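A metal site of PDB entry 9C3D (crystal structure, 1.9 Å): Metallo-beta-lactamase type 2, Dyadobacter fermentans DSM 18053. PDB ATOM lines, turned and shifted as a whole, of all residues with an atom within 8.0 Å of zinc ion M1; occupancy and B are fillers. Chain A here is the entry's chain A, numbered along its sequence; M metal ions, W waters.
Asp 87 touches zinc ion M1.
Four residues have an atom within 4 Å of zinc ion M1: His 83, His 85, Asp 87 and His 146.
The nearest printed residue that does not touch zinc ion M1 is Cys 165 (4.1 Å).
A ring nitrogen (NE2) of His 85 is in hydrogen-bond range of the side-chain carboxylate (OD2) of Asp 179 (2.5 Å).
The backbone NH (N) of His 146 is in hydrogen-bond range of the side-chain amide oxygen (OD1) of Asn 150 (2.9 Å).
ND1 of His 83 lies close to SG of Cys 88 (3.3 Å).
Zinc ion M1 is bound by water W1 (1.9 Å), NE2 of His 146 (2.2 Å), ND1 of His 85 (2.2 Å) and NE2 of His 83 (2.3 Å).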
ATOM      1  N   ASP A  53     -11.193  22.310  -6.196  1.00  0.00           N
ATOM      2  CA  ASP A  53      -9.870  21.683  -6.114  1.00  0.00           C
ATOM      3  C   ASP A  53      -9.190  21.992  -4.785  1.00  0.00           C
ATOM      4  O   ASP A  53      -9.191  23.132  -4.328  1.00  0.00           O
ATOM      5  CB  ASP A  53      -8.954  22.136  -7.267  1.00  0.00           C
ATOM      6  CG  ASP A  53      -9.248  21.421  -8.570  1.00  0.00           C
ATOM      7  OD1 ASP A  53     -10.235  20.655  -8.672  1.00  0.00           O
ATOM      8  OD2 ASP A  53      -8.471  21.641  -9.528  1.00  0.00           O
ATOM      9  N   THR A  82     -12.376  18.517  -9.184  1.00  0.00           N
ATOM     10  CA  THR A  82     -12.848  18.611 -10.568  1.00  0.00           C
ATOM     11  C   THR A  82     -12.302  17.523 -11.483  1.00  0.00           C
ATOM     12  O   THR A  82     -12.824  17.366 -12.595  1.00  0.00           O
ATOM     13  CB  THR A  82     -12.548  19.992 -11.161  1.00  0.00           C
ATOM     14  OG1 THR A  82     -11.144  20.249 -11.142  1.00  0.00           O
ATOM     15  CG2 THR A  82     -13.257  21.085 -10.354  1.00  0.00           C
ATOM     16  N   HIS A  83     -11.284  16.770 -11.063  1.00  0.00           N
ATOM     17  CA  HIS A  83     -11.004  15.445 -11.609  1.00  0.00           C
ATOM     18  C   HIS A  83     -10.094  14.715 -10.623  1.00  0.00           C
ATOM     19  O   HIS A  83      -9.805  15.220  -9.540  1.00  0.00           O
ATOM     20  CB  HIS A  83     -10.407  15.509 -13.034  1.00  0.00           C
ATOM     21  CG  HIS A  83      -9.049  16.113 -13.116  1.00  0.00           C
ATOM     22  ND1 HIS A  83      -8.844  17.468 -13.218  1.00  0.00           N
ATOM     23  CD2 HIS A  83      -7.817  15.548 -13.165  1.00  0.00           C
ATOM     24  CE1 HIS A  83      -7.547  17.717 -13.318  1.00  0.00           C
ATOM     25  NE2 HIS A  83      -6.904  16.568 -13.271  1.00  0.00           N
ATOM     26  N   PHE A  84      -9.666  13.501 -10.992  1.00  0.00           N
ATOM     27  CA  PHE A  84      -9.090  12.627  -9.985  1.00  0.00           C
ATOM     28  C   PHE A  84      -7.617  12.887  -9.708  1.00  0.00           C
ATOM     29  O   PHE A  84      -7.096  12.335  -8.729  1.00  0.00           O
ATOM     30  CB  PHE A  84      -9.297  11.150 -10.384  1.00  0.00           C
ATOM     31  CG  PHE A  84      -8.375  10.655 -11.481  1.00  0.00           C
ATOM     32  CD1 PHE A  84      -8.710  10.824 -12.814  1.00  0.00           C
ATOM     33  CD2 PHE A  84      -7.198   9.970 -11.174  1.00  0.00           C
ATOM     34  CE1 PHE A  84      -7.877  10.349 -13.827  1.00  0.00           C
ATOM     35  CE2 PHE A  84      -6.359   9.489 -12.177  1.00  0.00           C
ATOM     36  CZ  PHE A  84      -6.699   9.679 -13.504  1.00  0.00           C
ATOM     37  N   HIS A  85      -6.934  13.705 -10.500  1.00  0.00           N
ATOM     38  CA  HIS A  85      -5.496  13.890 -10.332  1.00  0.00           C
ATOM     39  C   HIS A  85      -5.171  14.620  -9.020  1.00  0.00           C
ATOM     40  O   HIS A  85      -6.026  15.243  -8.392  1.00  0.00           O
ATOM     41  CB  HIS A  85      -4.920  14.636 -11.525  1.00  0.00           C
ATOM     42  CG  HIS A  85      -4.770  13.786 -12.750  1.00  0.00           C
ATOM     43  ND1 HIS A  85      -4.637  14.318 -14.015  1.00  0.00           N
ATOM     44  CD2 HIS A  85      -4.713  12.444 -12.903  1.00  0.00           C
ATOM     45  CE1 HIS A  85      -4.526  13.353 -14.900  1.00  0.00           C
ATOM     46  NE2 HIS A  85      -4.559  12.198 -14.245  1.00  0.00           N
ATOM     47  N   GLU A  86      -3.894  14.534  -8.632  1.00  0.00           N
ATOM     48  CA  GLU A  86      -3.457  15.055  -7.337  1.00  0.00           C
ATOM     49  C   GLU A  86      -3.489  16.584  -7.241  1.00  0.00           C
ATOM     50  O   GLU A  86      -3.500  17.113  -6.128  1.00  0.00           O
ATOM     51  CB  GLU A  86      -2.053  14.542  -7.008  1.00  0.00           C
ATOM     52  CG  GLU A  86      -1.995  13.040  -6.723  1.00  0.00           C
ATOM     53  CD  GLU A  86      -0.674  12.610  -6.138  1.00  0.00           C
ATOM     54  OE1 GLU A  86       0.235  13.469  -6.008  1.00  0.00           O
ATOM     55  OE2 GLU A  86      -0.534  11.412  -5.795  1.00  0.00           O
ATOM     56  N   ASP A  87      -3.523  17.321  -8.366  1.00  0.00           N
ATOM     57  CA  ASP A  87      -3.731  18.764  -8.222  1.00  0.00           C
ATOM     58  C   ASP A  87      -5.198  19.124  -7.970  1.00  0.00           C
ATOM     59  O   ASP A  87      -5.558  20.315  -7.997  1.00  0.00           O
ATOM     60  CB  ASP A  87      -3.169  19.535  -9.428  1.00  0.00           C
ATOM     61  CG  ASP A  87      -3.637  19.014 -10.779  1.00  0.00           C
ATOM     62  OD1 ASP A  87      -3.754  17.774 -10.944  1.00  0.00           O
ATOM     63  OD2 ASP A  87      -3.857  19.850 -11.699  1.00  0.00           O
ATOM     64  N   CYS A  88      -6.048  18.110  -7.712  1.00  0.00           N
ATOM     65  CA  CYS A  88      -7.447  18.318  -7.353  1.00  0.00           C
ATOM     66  C   CYS A  88      -7.809  17.707  -5.996  1.00  0.00           C
ATOM     67  O   CYS A  88      -8.701  18.244  -5.336  1.00  0.00           O
ATOM     68  CB  CYS A  88      -8.389  17.727  -8.410  1.00  0.00           C
ATOM     69  SG  CYS A  88      -7.949  18.166 -10.095  1.00  0.00           S
ATOM     70  N   HIS A 146      -9.114  16.521 -20.808  1.00  0.00           N
ATOM     71  CA  HIS A 146      -7.888  16.307 -20.063  1.00  0.00           C
ATOM     72  C   HIS A 146      -7.904  14.934 -19.386  1.00  0.00           C
ATOM     73  O   HIS A 146      -6.881  14.246 -19.327  1.00  0.00           O
ATOM     74  CB  HIS A 146      -7.738  17.413 -19.028  1.00  0.00           C
ATOM     75  CG  HIS A 146      -6.552  17.224 -18.150  1.00  0.00           C
ATOM     76  ND1 HIS A 146      -5.267  17.436 -18.600  1.00  0.00           N
ATOM     77  CD2 HIS A 146      -6.443  16.860 -16.855  1.00  0.00           C
ATOM     78  CE1 HIS A 146      -4.408  17.196 -17.622  1.00  0.00           C
ATOM     79  NE2 HIS A 146      -5.095  16.833 -16.554  1.00  0.00           N
ATOM     80  N   THR A 147      -9.053  14.538 -18.860  1.00  0.00           N
ATOM     81  CA  THR A 147      -9.276  13.195 -18.361  1.00  0.00           C
ATOM     82  C   THR A 147     -10.687  12.788 -18.765  1.00  0.00           C
ATOM     83  O   THR A 147     -11.462  13.595 -19.264  1.00  0.00           O
ATOM     84  CB  THR A 147      -9.148  13.136 -16.841  1.00  0.00           C
ATOM     85  OG1 THR A 147     -10.089  14.055 -16.258  1.00  0.00           O
ATOM     86  CG2 THR A 147      -7.730  13.477 -16.389  1.00  0.00           C
ATOM     87  N   ASP A 149     -12.995  12.072 -16.726  1.00  0.00           N
ATOM     88  CA  ASP A 149     -13.911  12.475 -15.671  1.00  0.00           C
ATOM     89  C   ASP A 149     -14.009  13.988 -15.435  1.00  0.00           C
ATOM     90  O   ASP A 149     -14.793  14.413 -14.582  1.00  0.00           O
ATOM     91  CB  ASP A 149     -13.512  11.785 -14.356  1.00  0.00           C
ATOM     92  CG  ASP A 149     -12.123  12.206 -13.875  1.00  0.00           C
ATOM     93  OD1 ASP A 149     -11.214  12.355 -14.721  1.00  0.00           O
ATOM     94  OD2 ASP A 149     -11.937  12.419 -12.646  1.00  0.00           O
ATOM     95  N   ASN A 150     -13.231  14.816 -16.138  1.00  0.00           N
ATOM     96  CA  ASN A 150     -13.070  16.203 -15.703  1.00  0.00           C
ATOM     97  C   ASN A 150     -14.378  16.998 -15.801  1.00  0.00           C
ATOM     98  O   ASN A 150     -15.140  16.855 -16.757  1.00  0.00           O
ATOM     99  CB  ASN A 150     -11.962  16.934 -16.489  1.00  0.00           C
ATOM    100  CG  ASN A 150     -12.023  16.717 -17.996  1.00  0.00           C
ATOM    101  OD1 ASN A 150     -10.995  16.820 -18.680  1.00  0.00           O
ATOM    102  ND2 ASN A 150     -13.216  16.443 -18.536  1.00  0.00           N
ATOM    103  N   GLY A 164     -10.512  24.230 -14.667  1.00  0.00           N
ATOM    104  CA  GLY A 164      -9.671  23.104 -14.358  1.00  0.00           C
ATOM    105  C   GLY A 164      -8.753  22.752 -15.512  1.00  0.00           C
ATOM    106  O   GLY A 164      -8.543  23.531 -16.446  1.00  0.00           O
ATOM    107  N   CYS A 165      -8.219  21.537 -15.461  1.00  0.00           N
ATOM    108  CA  CYS A 165      -7.198  21.219 -16.449  1.00  0.00           C
ATOM    109  C   CYS A 165      -7.778  20.933 -17.821  1.00  0.00           C
ATOM    110  O   CYS A 165      -7.003  20.803 -18.782  1.00  0.00           O
ATOM    111  CB  CYS A 165      -6.352  20.075 -15.923  1.00  0.00           C
ATOM    112  SG  CYS A 165      -5.705  20.498 -14.263  1.00  0.00           S
ATOM    113  N   LEU A 166      -9.111  20.886 -17.936  1.00  0.00           N
ATOM    114  CA  LEU A 166      -9.772  20.808 -19.234  1.00  0.00           C
ATOM    115  C   LEU A 166      -9.520  22.057 -20.058  1.00  0.00           C
ATOM    116  O   LEU A 166      -9.591  22.022 -21.290  1.00  0.00           O
ATOM    117  CB  LEU A 166     -11.274  20.611 -19.030  1.00  0.00           C
ATOM    118  CG  LEU A 166     -12.208  20.467 -20.249  1.00  0.00           C
ATOM    119  CD1 LEU A 166     -11.834  19.232 -21.101  1.00  0.00           C
ATOM    120  CD2 LEU A 166     -13.659  20.393 -19.813  1.00  0.00           C
ATOM    121  N   LYS A 168      -7.035  25.281 -20.959  1.00  0.00           N
ATOM    122  CA  LYS A 168      -5.651  25.721 -20.973  1.00  0.00           C
ATOM    123  C   LYS A 168      -5.562  27.237 -20.991  1.00  0.00           C
ATOM    124  O   LYS A 168      -6.422  27.909 -21.580  1.00  0.00           O
ATOM    125  CB  LYS A 168      -4.922  25.160 -22.203  1.00  0.00           C
ATOM    126  CG  LYS A 168      -4.914  23.650 -22.255  1.00  0.00           C
ATOM    127  CD  LYS A 168      -4.083  23.100 -21.092  1.00  0.00           C
ATOM    128  CE  LYS A 168      -3.925  21.589 -21.194  1.00  0.00           C
ATOM    129  NZ  LYS A 168      -3.039  21.106 -20.096  1.00  0.00           N
ATOM    130  N   ASN A 176       0.054  17.421 -20.029  1.00  0.00           N
ATOM    131  CA  ASN A 176       0.074  15.996 -19.711  1.00  0.00           C
ATOM    132  C   ASN A 176      -1.148  15.337 -20.334  1.00  0.00           C
ATOM    133  O   ASN A 176      -2.276  15.619 -19.928  1.00  0.00           O
ATOM    134  CB  ASN A 176       0.084  15.789 -18.197  1.00  0.00           C
ATOM    135  CG  ASN A 176      -0.291  14.371 -17.787  1.00  0.00           C
ATOM    136  OD1 ASN A 176       0.104  13.417 -18.430  1.00  0.00           O
ATOM    137  ND2 ASN A 176      -1.068  14.246 -16.705  1.00  0.00           N
ATOM    138  N   ASP A 179      -3.865  10.661 -19.469  1.00  0.00           N
ATOM    139  CA  ASP A 179      -5.218  10.183 -19.219  1.00  0.00           C
ATOM    140  C   ASP A 179      -6.233  10.826 -20.144  1.00  0.00           C
ATOM    141  O   ASP A 179      -7.449  10.708 -19.908  1.00  0.00           O
ATOM    142  CB  ASP A 179      -5.601  10.442 -17.755  1.00  0.00           C
ATOM    143  CG  ASP A 179      -4.727   9.673 -16.780  1.00  0.00           C
ATOM    144  OD1 ASP A 179      -4.517   8.470 -16.999  1.00  0.00           O
ATOM    145  OD2 ASP A 179      -4.192  10.268 -15.830  1.00  0.00           O
ATOM    146  N   GLY A 205      -6.727  25.245 -15.287  1.00  0.00           N
ATOM    147  CA  GLY A 205      -6.115  24.410 -14.268  1.00  0.00           C
ATOM    148  C   GLY A 205      -4.716  24.871 -13.907  1.00  0.00           C
ATOM    149  O   GLY A 205      -4.307  24.760 -12.747  1.00  0.00           O
ATOM    150  N   HIS A 206      -3.991  25.404 -14.891  1.00  0.00           N
ATOM    151  CA  HIS A 206      -2.663  25.962 -14.697  1.00  0.00           C
ATOM    152  C   HIS A 206      -2.509  27.225 -15.530  1.00  0.00           C
ATOM    153  O   HIS A 206      -2.915  27.261 -16.692  1.00  0.00           O
ATOM    154  CB  HIS A 206      -1.566  24.971 -15.100  1.00  0.00           C
ATOM    155  CG  HIS A 206      -1.769  23.589 -14.553  1.00  0.00           C
ATOM    156  ND1 HIS A 206      -1.250  23.181 -13.345  1.00  0.00           N
ATOM    157  CD2 HIS A 206      -2.429  22.521 -15.068  1.00  0.00           C
ATOM    158  CE1 HIS A 206      -1.585  21.922 -13.137  1.00  0.00           C
ATOM    159  NE2 HIS A 206      -2.303  21.493 -14.157  1.00  0.00           N
HETATM  160 ZN    ZN M   1      -4.896  16.526 -14.358  1.00  0.00          ZN
HETATM  161 ZN    ZN M   2      -3.634  19.634 -14.008  1.00  0.00          ZN
HETATM  162  O   HOH W   1      -3.644  17.606 -13.491  1.00  0.00           O
